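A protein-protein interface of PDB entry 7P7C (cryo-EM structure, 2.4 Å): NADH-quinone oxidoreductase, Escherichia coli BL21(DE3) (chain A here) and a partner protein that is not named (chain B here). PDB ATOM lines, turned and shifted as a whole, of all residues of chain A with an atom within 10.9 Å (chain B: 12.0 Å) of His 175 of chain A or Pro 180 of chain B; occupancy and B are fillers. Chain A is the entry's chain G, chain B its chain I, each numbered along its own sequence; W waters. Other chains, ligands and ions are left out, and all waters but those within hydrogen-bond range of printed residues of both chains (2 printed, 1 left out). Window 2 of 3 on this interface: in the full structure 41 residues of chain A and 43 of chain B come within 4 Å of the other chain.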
ATOM      1  N   ALA A  43     -41.572  15.786  34.681  1.00  0.00           N
ATOM      2  CA  ALA A  43     -40.351  15.160  34.186  1.00  0.00           C
ATOM      3  C   ALA A  43     -39.684  14.286  35.247  1.00  0.00           C
ATOM      4  O   ALA A  43     -39.503  13.088  35.038  1.00  0.00           O
ATOM      5  CB  ALA A  43     -39.376  16.229  33.683  1.00  0.00           C
ATOM      6  N   TRP A  93     -31.909   6.660  41.677  1.00  0.00           N
ATOM      7  CA  TRP A  93     -31.590   6.716  40.254  1.00  0.00           C
ATOM      8  C   TRP A  93     -30.845   7.993  39.905  1.00  0.00           C
ATOM      9  O   TRP A  93     -29.921   7.974  39.086  1.00  0.00           O
ATOM     10  CB  TRP A  93     -32.864   6.612  39.417  1.00  0.00           C
ATOM     11  CG  TRP A  93     -33.465   5.256  39.406  1.00  0.00           C
ATOM     12  CD1 TRP A  93     -32.804   4.070  39.386  1.00  0.00           C
ATOM     13  CD2 TRP A  93     -34.858   4.941  39.418  1.00  0.00           C
ATOM     14  NE1 TRP A  93     -33.697   3.031  39.384  1.00  0.00           N
ATOM     15  CE2 TRP A  93     -34.967   3.540  39.405  1.00  0.00           C
ATOM     16  CE3 TRP A  93     -36.026   5.708  39.440  1.00  0.00           C
ATOM     17  CZ2 TRP A  93     -36.196   2.889  39.411  1.00  0.00           C
ATOM     18  CZ3 TRP A  93     -37.242   5.061  39.450  1.00  0.00           C
ATOM     19  CH2 TRP A  93     -37.320   3.666  39.432  1.00  0.00           C
ATOM     20  N   LEU A  94     -31.239   9.116  40.510  1.00  0.00           N
ATOM     21  CA  LEU A  94     -30.490  10.351  40.309  1.00  0.00           C
ATOM     22  C   LEU A  94     -29.090  10.264  40.901  1.00  0.00           C
ATOM     23  O   LEU A  94     -28.167  10.918  40.407  1.00  0.00           O
ATOM     24  CB  LEU A  94     -31.244  11.532  40.916  1.00  0.00           C
ATOM     25  CG  LEU A  94     -32.569  11.883  40.247  1.00  0.00           C
ATOM     26  CD1 LEU A  94     -33.212  13.050  40.959  1.00  0.00           C
ATOM     27  CD2 LEU A  94     -32.359  12.189  38.777  1.00  0.00           C
ATOM     28  N   ASN A  97     -25.342   8.404  38.908  1.00  0.00           N
ATOM     29  CA  ASN A  97     -24.344   9.110  38.122  1.00  0.00           C
ATOM     30  C   ASN A  97     -23.826  10.371  38.794  1.00  0.00           C
ATOM     31  O   ASN A  97     -22.992  11.064  38.208  1.00  0.00           O
ATOM     32  CB  ASN A  97     -24.914   9.466  36.750  1.00  0.00           C
ATOM     33  CG  ASN A  97     -25.249   8.244  35.928  1.00  0.00           C
ATOM     34  OD1 ASN A  97     -24.451   7.319  35.821  1.00  0.00           O
ATOM     35  ND2 ASN A  97     -26.436   8.235  35.343  1.00  0.00           N
ATOM     36  N   ARG A 132     -21.550   8.272  34.541  1.00  0.00           N
ATOM     37  CA  ARG A 132     -21.369   9.084  33.349  1.00  0.00           C
ATOM     38  C   ARG A 132     -20.785  10.440  33.723  1.00  0.00           C
ATOM     39  O   ARG A 132     -21.021  10.967  34.812  1.00  0.00           O
ATOM     40  CB  ARG A 132     -22.694   9.256  32.600  1.00  0.00           C
ATOM     41  CG  ARG A 132     -23.759  10.089  33.312  1.00  0.00           C
ATOM     42  CD  ARG A 132     -23.873  11.486  32.723  1.00  0.00           C
ATOM     43  NE  ARG A 132     -24.757  12.357  33.488  1.00  0.00           N
ATOM     44  CZ  ARG A 132     -24.410  13.014  34.587  1.00  0.00           C
ATOM     45  NH1 ARG A 132     -23.200  12.900  35.109  1.00  0.00           N
ATOM     46  NH2 ARG A 132     -25.300  13.805  35.178  1.00  0.00           N
ATOM     47  N   THR A 133     -20.003  11.000  32.809  1.00  0.00           N
ATOM     48  CA  THR A 133     -19.367  12.286  33.024  1.00  0.00           C
ATOM     49  C   THR A 133     -19.618  13.186  31.825  1.00  0.00           C
ATOM     50  O   THR A 133     -20.003  12.731  30.748  1.00  0.00           O
ATOM     51  CB  THR A 133     -17.857  12.148  33.270  1.00  0.00           C
ATOM     52  OG1 THR A 133     -17.296  11.222  32.333  1.00  0.00           O
ATOM     53  CG2 THR A 133     -17.598  11.652  34.672  1.00  0.00           C
ATOM     54  N   HIS A 134     -19.404  14.480  32.035  1.00  0.00           N
ATOM     55  CA  HIS A 134     -19.613  15.478  31.003  1.00  0.00           C
ATOM     56  C   HIS A 134     -18.505  16.516  31.061  1.00  0.00           C
ATOM     57  O   HIS A 134     -18.012  16.859  32.136  1.00  0.00           O
ATOM     58  CB  HIS A 134     -20.966  16.175  31.163  1.00  0.00           C
ATOM     59  CG  HIS A 134     -22.135  15.323  30.788  1.00  0.00           C
ATOM     60  ND1 HIS A 134     -22.339  14.865  29.506  1.00  0.00           N
ATOM     61  CD2 HIS A 134     -23.169  14.856  31.524  1.00  0.00           C
ATOM     62  CE1 HIS A 134     -23.447  14.150  29.469  1.00  0.00           C
ATOM     63  NE2 HIS A 134     -23.971  14.131  30.680  1.00  0.00           N
ATOM     64  N   MET A 147     -21.732  20.168  34.476  1.00  0.00           N
ATOM     65  CA  MET A 147     -22.799  19.296  33.997  1.00  0.00           C
ATOM     66  C   MET A 147     -22.772  17.904  34.616  1.00  0.00           C
ATOM     67  O   MET A 147     -23.735  17.155  34.434  1.00  0.00           O
ATOM     68  CB  MET A 147     -22.735  19.189  32.470  1.00  0.00           C
ATOM     69  CG  MET A 147     -23.824  19.976  31.750  1.00  0.00           C
ATOM     70  SD  MET A 147     -25.537  19.448  31.963  1.00  0.00           S
ATOM     71  CE  MET A 147     -25.409  17.678  31.741  1.00  0.00           C
ATOM     72  N   CYS A 150     -25.771  17.400  37.011  1.00  0.00           N
ATOM     73  CA  CYS A 150     -27.120  17.565  36.492  1.00  0.00           C
ATOM     74  C   CYS A 150     -27.969  16.331  36.750  1.00  0.00           C
ATOM     75  O   CYS A 150     -27.511  15.197  36.616  1.00  0.00           O
ATOM     76  CB  CYS A 150     -27.068  17.873  35.000  1.00  0.00           C
ATOM     77  SG  CYS A 150     -28.666  18.057  34.223  1.00  0.00           S
ATOM     78  N   ILE A 151     -29.218  16.564  37.138  1.00  0.00           N
ATOM     79  CA  ILE A 151     -30.192  15.504  37.339  1.00  0.00           C
ATOM     80  C   ILE A 151     -31.241  15.495  36.239  1.00  0.00           C
ATOM     81  O   ILE A 151     -32.226  14.759  36.341  1.00  0.00           O
ATOM     82  CB  ILE A 151     -30.846  15.605  38.723  1.00  0.00           C
ATOM     83  CG1 ILE A 151     -31.564  16.944  38.873  1.00  0.00           C
ATOM     84  CG2 ILE A 151     -29.806  15.422  39.812  1.00  0.00           C
ATOM     85  CD1 ILE A 151     -32.265  17.114  40.174  1.00  0.00           C
ATOM     86  N   ALA A 152     -31.046  16.305  35.190  1.00  0.00           N
ATOM     87  CA  ALA A 152     -31.924  16.377  34.015  1.00  0.00           C
ATOM     88  C   ALA A 152     -33.368  16.681  34.404  1.00  0.00           C
ATOM     89  O   ALA A 152     -34.305  15.994  34.000  1.00  0.00           O
ATOM     90  CB  ALA A 152     -31.836  15.102  33.173  1.00  0.00           C
ATOM     91  N   CYS A 153     -33.539  17.715  35.216  1.00  0.00           N
ATOM     92  CA  CYS A 153     -34.859  18.112  35.674  1.00  0.00           C
ATOM     93  C   CYS A 153     -35.515  19.154  34.777  1.00  0.00           C
ATOM     94  O   CYS A 153     -36.674  19.505  35.014  1.00  0.00           O
ATOM     95  CB  CYS A 153     -34.771  18.640  37.104  1.00  0.00           C
ATOM     96  SG  CYS A 153     -34.200  20.329  37.238  1.00  0.00           S
ATOM     97  N   TYR A 154     -34.793  19.668  33.782  1.00  0.00           N
ATOM     98  CA  TYR A 154     -35.268  20.574  32.736  1.00  0.00           C
ATOM     99  C   TYR A 154     -35.712  21.936  33.260  1.00  0.00           C
ATOM    100  O   TYR A 154     -36.310  22.701  32.508  1.00  0.00           O
ATOM    101  CB  TYR A 154     -36.401  19.950  31.904  1.00  0.00           C
ATOM    102  CG  TYR A 154     -35.973  18.764  31.078  1.00  0.00           C
ATOM    103  CD1 TYR A 154     -35.868  17.504  31.646  1.00  0.00           C
ATOM    104  CD2 TYR A 154     -35.669  18.902  29.733  1.00  0.00           C
ATOM    105  CE1 TYR A 154     -35.471  16.419  30.903  1.00  0.00           C
ATOM    106  CE2 TYR A 154     -35.273  17.822  28.981  1.00  0.00           C
ATOM    107  CZ  TYR A 154     -35.175  16.583  29.572  1.00  0.00           C
ATOM    108  OH  TYR A 154     -34.783  15.496  28.834  1.00  0.00           O
ATOM    109  N   VAL A 171     -31.397  22.016  25.578  1.00  0.00           N
ATOM    110  CA  VAL A 171     -31.086  20.640  25.932  1.00  0.00           C
ATOM    111  C   VAL A 171     -30.662  19.919  24.658  1.00  0.00           C
ATOM    112  O   VAL A 171     -31.277  20.091  23.600  1.00  0.00           O
ATOM    113  CB  VAL A 171     -32.278  19.952  26.625  1.00  0.00           C
ATOM    114  CG1 VAL A 171     -33.565  20.127  25.835  1.00  0.00           C
ATOM    115  CG2 VAL A 171     -31.993  18.483  26.897  1.00  0.00           C
ATOM    116  N   TYR A 172     -29.578  19.160  24.748  1.00  0.00           N
ATOM    117  CA  TYR A 172     -28.988  18.481  23.612  1.00  0.00           C
ATOM    118  C   TYR A 172     -28.782  17.021  23.966  1.00  0.00           C
ATOM    119  O   TYR A 172     -28.767  16.639  25.137  1.00  0.00           O
ATOM    120  CB  TYR A 172     -27.658  19.130  23.210  1.00  0.00           C
ATOM    121  CG  TYR A 172     -27.711  20.626  23.306  1.00  0.00           C
ATOM    122  CD1 TYR A 172     -28.393  21.375  22.358  1.00  0.00           C
ATOM    123  CD2 TYR A 172     -27.117  21.292  24.365  1.00  0.00           C
ATOM    124  CE1 TYR A 172     -28.467  22.741  22.452  1.00  0.00           C
ATOM    125  CE2 TYR A 172     -27.183  22.657  24.465  1.00  0.00           C
ATOM    126  CZ  TYR A 172     -27.859  23.377  23.507  1.00  0.00           C
ATOM    127  OH  TYR A 172     -27.927  24.742  23.609  1.00  0.00           O
ATOM    128  N   GLY A 173     -28.635  16.207  22.941  1.00  0.00           N
ATOM    129  CA  GLY A 173     -28.373  14.808  23.144  1.00  0.00           C
ATOM    130  C   GLY A 173     -29.631  14.011  23.413  1.00  0.00           C
ATOM    131  O   GLY A 173     -30.752  14.384  23.064  1.00  0.00           O
ATOM    132  N   ALA A 174     -29.422  12.888  24.082  1.00  0.00           N
ATOM    133  CA  ALA A 174     -30.405  11.821  24.149  1.00  0.00           C
ATOM    134  C   ALA A 174     -30.256  11.143  25.504  1.00  0.00           C
ATOM    135  O   ALA A 174     -29.667  11.697  26.437  1.00  0.00           O
ATOM    136  CB  ALA A 174     -30.245  10.859  22.963  1.00  0.00           C
ATOM    137  N   HIS A 175     -30.689   9.891  25.560  1.00  0.00           N
ATOM    138  CA  HIS A 175     -31.232   9.148  26.690  1.00  0.00           C
ATOM    139  C   HIS A 175     -30.695   9.472  28.080  1.00  0.00           C
ATOM    140  O   HIS A 175     -31.374  10.154  28.844  1.00  0.00           O
ATOM    141  CB  HIS A 175     -30.923   7.685  26.383  1.00  0.00           C
ATOM    142  CG  HIS A 175     -29.648   7.516  25.605  1.00  0.00           C
ATOM    143  ND1 HIS A 175     -28.413   7.433  26.208  1.00  0.00           N
ATOM    144  CD2 HIS A 175     -29.414   7.471  24.271  1.00  0.00           C
ATOM    145  CE1 HIS A 175     -27.477   7.322  25.285  1.00  0.00           C
ATOM    146  NE2 HIS A 175     -28.057   7.343  24.100  1.00  0.00           N
ATOM    147  N   ASP A 176     -29.463   9.098  28.393  1.00  0.00           N
ATOM    148  CA  ASP A 176     -28.849   9.505  29.647  1.00  0.00           C
ATOM    149  C   ASP A 176     -27.692  10.451  29.405  1.00  0.00           C
ATOM    150  O   ASP A 176     -27.004  10.834  30.353  1.00  0.00           O
ATOM    151  CB  ASP A 176     -28.389   8.290  30.463  1.00  0.00           C
ATOM    152  CG  ASP A 176     -27.554   7.319  29.655  1.00  0.00           C
ATOM    153  OD1 ASP A 176     -27.455   7.490  28.424  1.00  0.00           O
ATOM    154  OD2 ASP A 176     -26.994   6.381  30.256  1.00  0.00           O
ATOM    155  N   ASN A 177     -27.474  10.835  28.151  1.00  0.00           N
ATOM    156  CA  ASN A 177     -26.470  11.810  27.765  1.00  0.00           C
ATOM    157  C   ASN A 177     -27.081  13.179  27.496  1.00  0.00           C
ATOM    158  O   ASN A 177     -26.531  13.952  26.706  1.00  0.00           O
ATOM    159  CB  ASN A 177     -25.712  11.310  26.536  1.00  0.00           C
ATOM    160  CG  ASN A 177     -24.237  11.617  26.597  1.00  0.00           C
ATOM    161  OD1 ASN A 177     -23.635  11.613  27.667  1.00  0.00           O
ATOM    162  ND2 ASN A 177     -23.644  11.889  25.444  1.00  0.00           N
ATOM    163  N   VAL A 178     -28.224  13.484  28.115  1.00  0.00           N
ATOM    164  CA  VAL A 178     -28.837  14.798  27.952  1.00  0.00           C
ATOM    165  C   VAL A 178     -27.940  15.858  28.570  1.00  0.00           C
ATOM    166  O   VAL A 178     -27.468  15.720  29.705  1.00  0.00           O
ATOM    167  CB  VAL A 178     -30.251  14.837  28.554  1.00  0.00           C
ATOM    168  CG1 VAL A 178     -31.252  14.215  27.608  1.00  0.00           C
ATOM    169  CG2 VAL A 178     -30.292  14.123  29.891  1.00  0.00           C
ATOM    170  N   TYR A 179     -27.693  16.916  27.813  1.00  0.00           N
ATOM    171  CA  TYR A 179     -26.744  17.954  28.171  1.00  0.00           C
ATOM    172  C   TYR A 179     -27.468  19.289  28.136  1.00  0.00           C
ATOM    173  O   TYR A 179     -28.141  19.602  27.155  1.00  0.00           O
ATOM    174  CB  TYR A 179     -25.567  17.944  27.196  1.00  0.00           C
ATOM    175  CG  TYR A 179     -24.367  18.739  27.625  1.00  0.00           C
ATOM    176  CD1 TYR A 179     -24.280  20.101  27.366  1.00  0.00           C
ATOM    177  CD2 TYR A 179     -23.304  18.123  28.264  1.00  0.00           C
ATOM    178  CE1 TYR A 179     -23.174  20.825  27.748  1.00  0.00           C
ATOM    179  CE2 TYR A 179     -22.201  18.835  28.644  1.00  0.00           C
ATOM    180  CZ  TYR A 179     -22.138  20.186  28.387  1.00  0.00           C
ATOM    181  OH  TYR A 179     -21.031  20.899  28.773  1.00  0.00           O
ATOM    182  N   PHE A 180     -27.330  20.076  29.190  1.00  0.00           N
ATOM    183  CA  PHE A 180     -28.028  21.349  29.286  1.00  0.00           C
ATOM    184  C   PHE A 180     -27.000  22.466  29.213  1.00  0.00           C
ATOM    185  O   PHE A 180     -26.083  22.525  30.036  1.00  0.00           O
ATOM    186  CB  PHE A 180     -28.849  21.423  30.574  1.00  0.00           C
ATOM    187  CG  PHE A 180     -29.977  20.434  30.625  1.00  0.00           C
ATOM    188  CD1 PHE A 180     -29.760  19.133  31.044  1.00  0.00           C
ATOM    189  CD2 PHE A 180     -31.253  20.799  30.234  1.00  0.00           C
ATOM    190  CE1 PHE A 180     -30.788  18.223  31.083  1.00  0.00           C
ATOM    191  CE2 PHE A 180     -32.288  19.889  30.274  1.00  0.00           C
ATOM    192  CZ  PHE A 180     -32.055  18.602  30.696  1.00  0.00           C
ATOM    193  N   ALA B 170     -16.933   6.820  34.043  1.00  0.00           N
ATOM    194  CA  ALA B 170     -16.753   6.562  32.625  1.00  0.00           C
ATOM    195  C   ALA B 170     -16.239   7.817  31.932  1.00  0.00           C
ATOM    196  O   ALA B 170     -16.362   8.931  32.442  1.00  0.00           O
ATOM    197  CB  ALA B 170     -18.063   6.104  31.987  1.00  0.00           C
ATOM    198  N   LYS B 171     -15.641   7.618  30.765  1.00  0.00           N
ATOM    199  CA  LYS B 171     -15.203   8.747  29.961  1.00  0.00           C
ATOM    200  C   LYS B 171     -16.417   9.524  29.457  1.00  0.00           C
ATOM    201  O   LYS B 171     -17.468   8.930  29.202  1.00  0.00           O
ATOM    202  CB  LYS B 171     -14.353   8.269  28.781  1.00  0.00           C
ATOM    203  CG  LYS B 171     -12.939   7.753  29.116  1.00  0.00           C
ATOM    204  CD  LYS B 171     -11.830   8.828  29.099  1.00  0.00           C
ATOM    205  CE  LYS B 171     -11.844   9.799  30.281  1.00  0.00           C
ATOM    206  NZ  LYS B 171     -10.661  10.701  30.298  1.00  0.00           N
ATOM    207  N   PRO B 172     -16.318  10.848  29.342  1.00  0.00           N
ATOM    208  CA  PRO B 172     -17.463  11.627  28.859  1.00  0.00           C
ATOM    209  C   PRO B 172     -17.785  11.313  27.408  1.00  0.00           C
ATOM    210  O   PRO B 172     -16.895  11.159  26.569  1.00  0.00           O
ATOM    211  CB  PRO B 172     -17.007  13.081  29.031  1.00  0.00           C
ATOM    212  CG  PRO B 172     -15.526  13.017  29.109  1.00  0.00           C
ATOM    213  CD  PRO B 172     -15.195  11.709  29.747  1.00  0.00           C
ATOM    214  N   ILE B 173     -19.077  11.208  27.123  1.00  0.00           N
ATOM    215  CA  ILE B 173     -19.580  10.979  25.777  1.00  0.00           C
ATOM    216  C   ILE B 173     -20.191  12.288  25.307  1.00  0.00           C
ATOM    217  O   ILE B 173     -21.172  12.771  25.883  1.00  0.00           O
ATOM    218  CB  ILE B 173     -20.603   9.839  25.731  1.00  0.00           C
ATOM    219  CG1 ILE B 173     -20.015   8.569  26.348  1.00  0.00           C
ATOM    220  CG2 ILE B 173     -21.046   9.585  24.302  1.00  0.00           C
ATOM    221  CD1 ILE B 173     -21.029   7.471  26.558  1.00  0.00           C
ATOM    222  N   ASP B 174     -19.606  12.871  24.269  1.00  0.00           N
ATOM    223  CA  ASP B 174     -20.100  14.130  23.743  1.00  0.00           C
ATOM    224  C   ASP B 174     -21.403  13.893  22.984  1.00  0.00           C
ATOM    225  O   ASP B 174     -21.627  12.823  22.415  1.00  0.00           O
ATOM    226  CB  ASP B 174     -19.036  14.765  22.848  1.00  0.00           C
ATOM    227  CG  ASP B 174     -19.473  16.082  22.260  1.00  0.00           C
ATOM    228  OD1 ASP B 174     -19.377  17.110  22.958  1.00  0.00           O
ATOM    229  OD2 ASP B 174     -19.904  16.090  21.097  1.00  0.00           O
ATOM    230  N   VAL B 175     -22.282  14.899  22.999  1.00  0.00           N
ATOM    231  CA  VAL B 175     -23.609  14.744  22.408  1.00  0.00           C
ATOM    232  C   VAL B 175     -23.568  14.665  20.888  1.00  0.00           C
ATOM    233  O   VAL B 175     -24.547  14.236  20.271  1.00  0.00           O
ATOM    234  CB  VAL B 175     -24.544  15.885  22.850  1.00  0.00           C
ATOM    235  CG1 VAL B 175     -24.925  15.720  24.305  1.00  0.00           C
ATOM    236  CG2 VAL B 175     -23.891  17.236  22.608  1.00  0.00           C
ATOM    237  N   LYS B 176     -22.464  15.059  20.263  1.00  0.00           N
ATOM    238  CA  LYS B 176     -22.318  14.959  18.820  1.00  0.00           C
ATOM    239  C   LYS B 176     -21.738  13.624  18.375  1.00  0.00           C
ATOM    240  O   LYS B 176     -21.390  13.479  17.200  1.00  0.00           O
ATOM    241  CB  LYS B 176     -21.450  16.103  18.294  1.00  0.00           C
ATOM    242  CG  LYS B 176     -21.828  17.467  18.832  1.00  0.00           C
ATOM    243  CD  LYS B 176     -20.833  18.521  18.392  1.00  0.00           C
ATOM    244  CE  LYS B 176     -21.085  19.845  19.090  1.00  0.00           C
ATOM    245  NZ  LYS B 176     -20.973  19.728  20.573  1.00  0.00           N
ATOM    246  N   SER B 177     -21.620  12.656  19.282  1.00  0.00           N
ATOM    247  CA  SER B 177     -21.067  11.355  18.935  1.00  0.00           C
ATOM    248  C   SER B 177     -22.006  10.594  18.006  1.00  0.00           C
ATOM    249  O   SER B 177     -23.230  10.721  18.080  1.00  0.00           O
ATOM    250  CB  SER B 177     -20.801  10.530  20.193  1.00  0.00           C
ATOM    251  OG  SER B 177     -21.920   9.725  20.521  1.00  0.00           O
ATOM    252  N   LEU B 178     -21.411   9.792  17.123  1.00  0.00           N
ATOM    253  CA  LEU B 178     -22.169   9.078  16.106  1.00  0.00           C
ATOM    254  C   LEU B 178     -22.903   7.862  16.650  1.00  0.00           C
ATOM    255  O   LEU B 178     -23.843   7.387  16.005  1.00  0.00           O
ATOM    256  CB  LEU B 178     -21.239   8.642  14.977  1.00  0.00           C
ATOM    257  CG  LEU B 178     -20.418   9.759  14.341  1.00  0.00           C
ATOM    258  CD1 LEU B 178     -19.293   9.179  13.507  1.00  0.00           C
ATOM    259  CD2 LEU B 178     -21.311  10.655  13.505  1.00  0.00           C
ATOM    260  N   LEU B 179     -22.497   7.349  17.804  1.00  0.00           N
ATOM    261  CA  LEU B 179     -23.133   6.164  18.352  1.00  0.00           C
ATOM    262  C   LEU B 179     -24.525   6.507  18.881  1.00  0.00           C
ATOM    263  O   LEU B 179     -24.729   7.592  19.431  1.00  0.00           O
ATOM    264  CB  LEU B 179     -22.275   5.569  19.468  1.00  0.00           C
ATOM    265  CG  LEU B 179     -20.990   4.889  18.999  1.00  0.00           C
ATOM    266  CD1 LEU B 179     -20.086   4.575  20.177  1.00  0.00           C
ATOM    267  CD2 LEU B 179     -21.314   3.630  18.217  1.00  0.00           C
ATOM    268  N   PRO B 180     -25.507   5.605  18.722  1.00  0.00           N
ATOM    269  CA  PRO B 180     -26.873   5.839  19.206  1.00  0.00           C
ATOM    270  C   PRO B 180     -26.962   5.898  20.730  1.00  0.00           C
ATOM    271  O   PRO B 180     -26.075   5.377  21.408  1.00  0.00           O
ATOM    272  CB  PRO B 180     -27.651   4.633  18.669  1.00  0.00           C
ATOM    273  CG  PRO B 180     -26.802   4.064  17.586  1.00  0.00           C
ATOM    274  CD  PRO B 180     -25.396   4.336  17.987  1.00  0.00           C
HETATM  275  O   HOH W   1     -19.830   9.273  30.252  1.00  0.00           O
HETATM  276  O   HOH W   2     -21.370  11.490  29.117  1.00  0.00           O
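OG1 of Thr 133 of chain A sits at hydrogen-bond distance from O of Ala 170 of chain B (2.5 Å).
OG1 of Thr 133 of chain A lies close to N of Pro 172 of chain B (3.2 Å).
ND2 of Asn 177 of chain A sits at hydrogen-bond distance from O of Ile 173 of chain B, 2.7 Å away.
The side-chain carboxylate (OD2) of Asp 174 of chain B lies within salt-bridge range of the side-chain amino group (NZ) of Lys 176 of chain B (3.8 Å).
The side-chain carboxylate (OD1) of Asp 176 of chain A is in hydrogen-bond range of a ring nitrogen (ND1) of His 175 of chain A (2.4 Å).
O of Tyr 179 of chain A sits at hydrogen-bond distance from N of Tyr 172 of chain A, at 2.8 Å.
OG1 of Thr 133 of chain A touches C of Lys 171 of chain B, at 3.5 Å.
Gly 173 of chain A touches Val 175 of chain B.
Pro 180 of chain B touches His 175 of chain A.
Asp 174 of chain B touches Asn 177 of chain A.
Val 175 of chain B touches Asn 177 of chain A (CG1 to O, 3.4 Å).
CB of Tyr 179 of chain A touches CG1 of Val 175 of chain B, 3.7 Å away.
Of the printed residues of chain B, Thr 133 of chain A touches Ala 170, Lys 171 and Pro 172.
No residue of chain B comes within 4 Å of Ala 174 of chain A.
Of chain B, only Pro 180 (3.8 Å) comes within 4 Å of His 175 of chain A.
Asp 176 of chain A touches none of the printed residues of chain B.
Of chain B, only Ile 173 (2.7 Å), Asp 174 (3.8 Å) and Val 175 (3.4 Å) come within 4 Å of Asn 177 of chain A.
No residue of chain B comes within 4 Å of Val 178 of chain A.
Of the printed residues of chain B, Tyr 179 of chain A touches Val 175.
Of the printed residues of chain A, Lys 171 of chain B touches Thr 133.
Of the printed residues of chain A, Ile 173 of chain B touches Asn 177.
No residue of chain A comes within 4 Å of Leu 179 of chain B.
Pro 180 of chain B touches just one residue of chain A: His 175.
The nearest residue of chain B that does not touch His 175 of chain A is Leu 179 of chain B (5.7 Å).
The nearest printed residue of chain A that does not touch Asp 174 of chain B is His 134 of chain A (6.2 Å).
Of the 23 printed residues of chain A, 5 touch a printed residue of chain B.
Along chain A the printed residues that touch a printed residue of chain B span positions 133 to 179.
Hydrophobic or aromatic side chains of chain B within 4 Å of the printed part of chain A: Pro 172, Ile 173 and Val 175.
Among the printed residues, no Asp or Glu carboxylate lies within 4 Å of a Lys or Arg side-chain nitrogen of the other chain.
Water W2 lies within hydrogen-bond range of O of Thr 133 of chain A (2.5 Å), OD1 of Asn 177 of chain A (2.7 Å) and N of Ile 173 of chain B (3.1 Å).
Water W1 lies within hydrogen-bond range of the backbone carbonyl oxygen (O) of Lys 171 of chain B (2.6 Å) and the backbone NH (N) of Thr 133 of chain A (3.1 Å).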
